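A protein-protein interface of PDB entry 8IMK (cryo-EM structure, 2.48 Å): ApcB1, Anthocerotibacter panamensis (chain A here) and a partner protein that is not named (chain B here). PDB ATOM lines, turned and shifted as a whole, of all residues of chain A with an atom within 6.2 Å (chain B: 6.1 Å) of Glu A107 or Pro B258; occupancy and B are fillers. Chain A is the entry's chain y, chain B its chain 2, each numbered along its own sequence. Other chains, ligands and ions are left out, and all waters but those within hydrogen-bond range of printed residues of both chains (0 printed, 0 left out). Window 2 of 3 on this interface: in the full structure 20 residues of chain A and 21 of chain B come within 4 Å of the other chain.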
ATOM      1  N   MET A   1     -24.870  13.290 -10.562  1.00  0.00           N
ATOM      2  CA  MET A   1     -23.551  12.747 -10.858  1.00  0.00           C
ATOM      3  C   MET A   1     -23.370  11.340 -10.306  1.00  0.00           C
ATOM      4  O   MET A   1     -24.131  10.889  -9.454  1.00  0.00           O
ATOM      5  CB  MET A   1     -22.455  13.648 -10.295  1.00  0.00           C
ATOM      6  CG  MET A   1     -22.464  13.724  -8.785  1.00  0.00           C
ATOM      7  SD  MET A   1     -21.163  14.757  -8.101  1.00  0.00           S
ATOM      8  CE  MET A   1     -19.749  13.708  -8.405  1.00  0.00           C
ATOM      9  N   THR A 102     -15.996  10.577 -14.281  1.00  0.00           N
ATOM     10  CA  THR A 102     -15.961  11.881 -14.934  1.00  0.00           C
ATOM     11  C   THR A 102     -17.333  12.523 -15.090  1.00  0.00           C
ATOM     12  O   THR A 102     -17.434  13.570 -15.730  1.00  0.00           O
ATOM     13  CB  THR A 102     -15.301  11.776 -16.310  1.00  0.00           C
ATOM     14  OG1 THR A 102     -16.010  10.827 -17.114  1.00  0.00           O
ATOM     15  CG2 THR A 102     -13.861  11.343 -16.182  1.00  0.00           C
ATOM     16  N   SER A 103     -18.387  11.930 -14.527  1.00  0.00           N
ATOM     17  CA  SER A 103     -19.731  12.451 -14.755  1.00  0.00           C
ATOM     18  C   SER A 103     -19.915  13.839 -14.148  1.00  0.00           C
ATOM     19  O   SER A 103     -20.756  14.615 -14.612  1.00  0.00           O
ATOM     20  CB  SER A 103     -20.775  11.478 -14.206  1.00  0.00           C
ATOM     21  OG  SER A 103     -20.818  11.500 -12.794  1.00  0.00           O
ATOM     22  N   VAL A 104     -19.150  14.170 -13.108  1.00  0.00           N
ATOM     23  CA  VAL A 104     -19.254  15.505 -12.524  1.00  0.00           C
ATOM     24  C   VAL A 104     -18.807  16.557 -13.531  1.00  0.00           C
ATOM     25  O   VAL A 104     -19.356  17.663 -13.587  1.00  0.00           O
ATOM     26  CB  VAL A 104     -18.454  15.586 -11.208  1.00  0.00           C
ATOM     27  CG1 VAL A 104     -16.973  15.416 -11.456  1.00  0.00           C
ATOM     28  CG2 VAL A 104     -18.727  16.891 -10.491  1.00  0.00           C
ATOM     29  N   ILE A 105     -17.812  16.223 -14.353  1.00  0.00           N
ATOM     30  CA  ILE A 105     -17.339  17.149 -15.375  1.00  0.00           C
ATOM     31  C   ILE A 105     -18.383  17.308 -16.470  1.00  0.00           C
ATOM     32  O   ILE A 105     -18.605  18.411 -16.983  1.00  0.00           O
ATOM     33  CB  ILE A 105     -15.980  16.674 -15.922  1.00  0.00           C
ATOM     34  CG1 ILE A 105     -14.911  16.807 -14.838  1.00  0.00           C
ATOM     35  CG2 ILE A 105     -15.574  17.470 -17.145  1.00  0.00           C
ATOM     36  CD1 ILE A 105     -13.679  15.989 -15.087  1.00  0.00           C
ATOM     37  N   ASP A 106     -19.059  16.219 -16.832  1.00  0.00           N
ATOM     38  CA  ASP A 106     -20.137  16.300 -17.812  1.00  0.00           C
ATOM     39  C   ASP A 106     -21.296  17.145 -17.301  1.00  0.00           C
ATOM     40  O   ASP A 106     -21.875  17.941 -18.047  1.00  0.00           O
ATOM     41  CB  ASP A 106     -20.630  14.901 -18.155  1.00  0.00           C
ATOM     42  CG  ASP A 106     -19.560  14.046 -18.766  1.00  0.00           C
ATOM     43  OD1 ASP A 106     -18.909  13.274 -18.034  1.00  0.00           O
ATOM     44  OD2 ASP A 106     -19.376  14.140 -19.988  1.00  0.00           O
ATOM     45  N   GLU A 107     -21.669  16.962 -16.036  1.00  0.00           N
ATOM     46  CA  GLU A 107     -22.842  17.646 -15.510  1.00  0.00           C
ATOM     47  C   GLU A 107     -22.566  19.118 -15.246  1.00  0.00           C
ATOM     48  O   GLU A 107     -23.411  19.972 -15.531  1.00  0.00           O
ATOM     49  CB  GLU A 107     -23.316  16.960 -14.231  1.00  0.00           C
ATOM     50  CG  GLU A 107     -23.836  15.554 -14.436  1.00  0.00           C
ATOM     51  CD  GLU A 107     -25.111  15.519 -15.247  1.00  0.00           C
ATOM     52  OE1 GLU A 107     -25.904  16.479 -15.156  1.00  0.00           O
ATOM     53  OE2 GLU A 107     -25.320  14.529 -15.978  1.00  0.00           O
ATOM     54  N   ARG A 108     -21.395  19.437 -14.697  1.00  0.00           N
ATOM     55  CA  ARG A 108     -21.135  20.770 -14.179  1.00  0.00           C
ATOM     56  C   ARG A 108     -20.211  21.614 -15.044  1.00  0.00           C
ATOM     57  O   ARG A 108     -20.210  22.837 -14.894  1.00  0.00           O
ATOM     58  CB  ARG A 108     -20.533  20.677 -12.770  1.00  0.00           C
ATOM     59  CG  ARG A 108     -21.442  20.066 -11.712  1.00  0.00           C
ATOM     60  CD  ARG A 108     -22.603  20.972 -11.391  1.00  0.00           C
ATOM     61  NE  ARG A 108     -23.417  20.451 -10.297  1.00  0.00           N
ATOM     62  CZ  ARG A 108     -24.471  19.659 -10.460  1.00  0.00           C
ATOM     63  NH1 ARG A 108     -24.845  19.294 -11.679  1.00  0.00           N
ATOM     64  NH2 ARG A 108     -25.151  19.235  -9.405  1.00  0.00           N
ATOM     65  N   VAL A 109     -19.436  21.009 -15.939  1.00  0.00           N
ATOM     66  CA  VAL A 109     -18.453  21.742 -16.713  1.00  0.00           C
ATOM     67  C   VAL A 109     -18.781  21.779 -18.200  1.00  0.00           C
ATOM     68  O   VAL A 109     -18.790  22.863 -18.792  1.00  0.00           O
ATOM     69  CB  VAL A 109     -17.045  21.157 -16.482  1.00  0.00           C
ATOM     70  CG1 VAL A 109     -16.035  21.829 -17.381  1.00  0.00           C
ATOM     71  CG2 VAL A 109     -16.654  21.300 -15.043  1.00  0.00           C
ATOM     72  N   LEU A 110     -19.057  20.636 -18.820  1.00  0.00           N
ATOM     73  CA  LEU A 110     -19.246  20.544 -20.258  1.00  0.00           C
ATOM     74  C   LEU A 110     -20.709  20.689 -20.670  1.00  0.00           C
ATOM     75  O   LEU A 110     -21.068  20.325 -21.792  1.00  0.00           O
ATOM     76  CB  LEU A 110     -18.673  19.223 -20.769  1.00  0.00           C
ATOM     77  CG  LEU A 110     -17.197  18.982 -20.443  1.00  0.00           C
ATOM     78  CD1 LEU A 110     -16.755  17.598 -20.866  1.00  0.00           C
ATOM     79  CD2 LEU A 110     -16.311  20.030 -21.081  1.00  0.00           C
ATOM     80  N   ASN A 111     -21.558  21.213 -19.788  1.00  0.00           N
ATOM     81  CA  ASN A 111     -22.975  21.394 -20.094  1.00  0.00           C
ATOM     82  C   ASN A 111     -23.149  22.699 -20.867  1.00  0.00           C
ATOM     83  O   ASN A 111     -23.631  23.711 -20.357  1.00  0.00           O
ATOM     84  CB  ASN A 111     -23.804  21.376 -18.817  1.00  0.00           C
ATOM     85  CG  ASN A 111     -23.207  22.226 -17.724  1.00  0.00           C
ATOM     86  OD1 ASN A 111     -22.040  22.077 -17.381  1.00  0.00           O
ATOM     87  ND2 ASN A 111     -24.011  23.112 -17.158  1.00  0.00           N
ATOM     88  N   ARG B 255     -26.207  11.882 -21.952  1.00  0.00           N
ATOM     89  CA  ARG B 255     -26.372  11.656 -20.525  1.00  0.00           C
ATOM     90  C   ARG B 255     -27.793  11.986 -20.088  1.00  0.00           C
ATOM     91  O   ARG B 255     -28.481  12.811 -20.695  1.00  0.00           O
ATOM     92  CB  ARG B 255     -25.373  12.497 -19.732  1.00  0.00           C
ATOM     93  CG  ARG B 255     -25.786  13.951 -19.585  1.00  0.00           C
ATOM     94  CD  ARG B 255     -24.656  14.821 -19.070  1.00  0.00           C
ATOM     95  NE  ARG B 255     -24.726  16.158 -19.649  1.00  0.00           N
ATOM     96  CZ  ARG B 255     -25.301  17.202 -19.067  1.00  0.00           C
ATOM     97  NH1 ARG B 255     -25.316  18.378 -19.677  1.00  0.00           N
ATOM     98  NH2 ARG B 255     -25.856  17.073 -17.872  1.00  0.00           N
ATOM     99  N   SER B 256     -28.237  11.314 -19.033  1.00  0.00           N
ATOM    100  CA  SER B 256     -29.530  11.627 -18.449  1.00  0.00           C
ATOM    101  C   SER B 256     -29.420  12.871 -17.580  1.00  0.00           C
ATOM    102  O   SER B 256     -28.447  13.051 -16.843  1.00  0.00           O
ATOM    103  CB  SER B 256     -30.041  10.449 -17.625  1.00  0.00           C
ATOM    104  OG  SER B 256     -29.276  10.292 -16.446  1.00  0.00           O
ATOM    105  N   LEU B 257     -30.418  13.736 -17.677  1.00  0.00           N
ATOM    106  CA  LEU B 257     -30.370  14.951 -16.884  1.00  0.00           C
ATOM    107  C   LEU B 257     -31.152  14.770 -15.594  1.00  0.00           C
ATOM    108  O   LEU B 257     -32.220  14.150 -15.600  1.00  0.00           O
ATOM    109  CB  LEU B 257     -30.954  16.126 -17.665  1.00  0.00           C
ATOM    110  CG  LEU B 257     -30.269  16.468 -18.986  1.00  0.00           C
ATOM    111  CD1 LEU B 257     -31.233  17.197 -19.888  1.00  0.00           C
ATOM    112  CD2 LEU B 257     -29.035  17.307 -18.741  1.00  0.00           C
ATOM    113  N   PRO B 258     -30.643  15.273 -14.473  1.00  0.00           N
ATOM    114  CA  PRO B 258     -31.410  15.196 -13.228  1.00  0.00           C
ATOM    115  C   PRO B 258     -32.744  15.903 -13.371  1.00  0.00           C
ATOM    116  O   PRO B 258     -32.849  16.964 -13.991  1.00  0.00           O
ATOM    117  CB  PRO B 258     -30.520  15.898 -12.197  1.00  0.00           C
ATOM    118  CG  PRO B 258     -29.216  16.128 -12.841  1.00  0.00           C
ATOM    119  CD  PRO B 258     -29.283  15.800 -14.290  1.00  0.00           C
ATOM    120  N   LEU B 259     -33.775  15.292 -12.793  1.00  0.00           N
ATOM    121  CA  LEU B 259     -35.117  15.845 -12.907  1.00  0.00           C
ATOM    122  C   LEU B 259     -35.215  17.174 -12.170  1.00  0.00           C
ATOM    123  O   LEU B 259     -35.872  18.110 -12.636  1.00  0.00           O
ATOM    124  CB  LEU B 259     -36.129  14.845 -12.355  1.00  0.00           C
ATOM    125  CG  LEU B 259     -36.247  13.539 -13.142  1.00  0.00           C
ATOM    126  CD1 LEU B 259     -37.177  12.571 -12.430  1.00  0.00           C
ATOM    127  CD2 LEU B 259     -36.700  13.774 -14.565  1.00  0.00           C
ATOM    128  N   VAL B 260     -34.562  17.266 -11.019  1.00  0.00           N
ATOM    129  CA  VAL B 260     -34.527  18.469 -10.193  1.00  0.00           C
ATOM    130  C   VAL B 260     -33.083  18.693  -9.772  1.00  0.00           C
ATOM    131  O   VAL B 260     -32.304  17.736  -9.671  1.00  0.00           O
ATOM    132  CB  VAL B 260     -35.442  18.321  -8.955  1.00  0.00           C
ATOM    133  CG1 VAL B 260     -34.929  17.230  -8.028  1.00  0.00           C
ATOM    134  CG2 VAL B 260     -35.661  19.627  -8.217  1.00  0.00           C
ATOM    135  N   PRO B 261     -32.680  19.947  -9.562  1.00  0.00           N
ATOM    136  CA  PRO B 261     -31.337  20.185  -9.033  1.00  0.00           C
ATOM    137  C   PRO B 261     -31.138  19.460  -7.714  1.00  0.00           C
ATOM    138  O   PRO B 261     -32.071  19.270  -6.932  1.00  0.00           O
ATOM    139  CB  PRO B 261     -31.292  21.703  -8.848  1.00  0.00           C
ATOM    140  CG  PRO B 261     -32.202  22.202  -9.874  1.00  0.00           C
ATOM    141  CD  PRO B 261     -33.322  21.214  -9.947  1.00  0.00           C
ATOM    142  N   GLU B 262     -29.896  19.033  -7.488  1.00  0.00           N
ATOM    143  CA  GLU B 262     -29.597  18.209  -6.323  1.00  0.00           C
ATOM    144  C   GLU B 262     -29.921  18.942  -5.029  1.00  0.00           C
ATOM    145  O   GLU B 262     -30.176  18.312  -3.996  1.00  0.00           O
ATOM    146  CB  GLU B 262     -28.132  17.785  -6.352  1.00  0.00           C
ATOM    147  CG  GLU B 262     -27.778  16.891  -7.525  1.00  0.00           C
ATOM    148  CD  GLU B 262     -28.427  15.524  -7.441  1.00  0.00           C
ATOM    149  OE1 GLU B 262     -28.588  15.006  -6.315  1.00  0.00           O
ATOM    150  OE2 GLU B 262     -28.780  14.968  -8.501  1.00  0.00           O
ATOM    151  N   TYR B 391     -35.015  24.881 -12.020  1.00  0.00           N
ATOM    152  CA  TYR B 391     -35.625  24.109 -13.092  1.00  0.00           C
ATOM    153  C   TYR B 391     -36.155  22.790 -12.546  1.00  0.00           C
ATOM    154  O   TYR B 391     -35.703  22.313 -11.506  1.00  0.00           O
ATOM    155  CB  TYR B 391     -34.622  23.870 -14.222  1.00  0.00           C
ATOM    156  CG  TYR B 391     -33.552  22.840 -13.937  1.00  0.00           C
ATOM    157  CD1 TYR B 391     -33.791  21.485 -14.133  1.00  0.00           C
ATOM    158  CD2 TYR B 391     -32.293  23.224 -13.510  1.00  0.00           C
ATOM    159  CE1 TYR B 391     -32.818  20.550 -13.886  1.00  0.00           C
ATOM    160  CE2 TYR B 391     -31.312  22.293 -13.264  1.00  0.00           C
ATOM    161  CZ  TYR B 391     -31.580  20.960 -13.450  1.00  0.00           C
ATOM    162  OH  TYR B 391     -30.602  20.028 -13.205  1.00  0.00           O
ATOM    163  N   LEU B 393     -37.412  19.183 -14.539  1.00  0.00           N
ATOM    164  CA  LEU B 393     -37.663  18.484 -15.798  1.00  0.00           C
ATOM    165  C   LEU B 393     -38.668  17.357 -15.572  1.00  0.00           C
ATOM    166  O   LEU B 393     -38.391  16.174 -15.755  1.00  0.00           O
ATOM    167  CB  LEU B 393     -36.359  17.964 -16.379  1.00  0.00           C
ATOM    168  CG  LEU B 393     -35.323  19.042 -16.674  1.00  0.00           C
ATOM    169  CD1 LEU B 393     -34.052  18.412 -17.199  1.00  0.00           C
ATOM    170  CD2 LEU B 393     -35.887  20.052 -17.648  1.00  0.00           C
ATOM    171  N   VAL B 416     -31.644  23.543 -20.091  1.00  0.00           N
ATOM    172  CA  VAL B 416     -30.844  22.981 -19.004  1.00  0.00           C
ATOM    173  C   VAL B 416     -29.641  22.223 -19.556  1.00  0.00           C
ATOM    174  O   VAL B 416     -28.552  22.254 -18.975  1.00  0.00           O
ATOM    175  CB  VAL B 416     -31.721  22.088 -18.106  1.00  0.00           C
ATOM    176  CG1 VAL B 416     -30.869  21.236 -17.193  1.00  0.00           C
ATOM    177  CG2 VAL B 416     -32.671  22.931 -17.291  1.00  0.00           C
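The backbone carbonyl oxygen (O) of Glu A107 sits close to the side-chain amide oxygen (OD1) of Asn A111 (3.1 Å).
The backbone carbonyl oxygen of Arg A108 sits close to the side-chain amide oxygen of Asn A111 (3.2 Å).
The backbone NH (N) of Val A109 lies within hydrogen-bond range of the side-chain amide oxygen (OD1) of Asn A111.
The side-chain carboxylate (OE1) of Glu A107 lies within salt-bridge range of the guanidinium group (NH2) of Arg B255 (2.8 Å).
Printed residues of chain B that touch a printed residue of chain A: Arg B255, Ser B256, Pro B258 and Glu B262.
Among the printed residues, Asp or Glu carboxylates within 4 Å of a Lys or Arg side-chain nitrogen of the other chain: Glu A107 with Arg B255 (2.8 Å).
Among the printed residues, pairs that only touch across the chains: Asp A106 with Arg B255, Glu A107 with Ser B256, Glu A107 with Pro B258, Arg A108 with Glu B262 and Asn A111 with Arg B255.
Of the printed residues of chain A, Pro B258 touches Glu A107.
Printed residues of chain A within 4 Å of Ser B256: Glu A107.
Printed residues of chain B within 4 Å of Asp A106: Arg B255 (3.7 Å).
Printed residues of chain B within 4 Å of Arg A108: Glu B262.
Of the printed residues of chain A, Arg B255 touches Asp A106 (3.7 Å), Glu A107 (2.8 Å) and Asn A111 (3.5 Å).
Printed residues of chain B within 4 Å of Asn A111: Arg B255 (3.5 Å).
Val B416 touches none of the printed residues of chain A.
Ser A103 touches none of the printed residues of chain B.
The nearest residue of chain A that does not touch Pro B258 is Arg A108 (5.5 Å).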
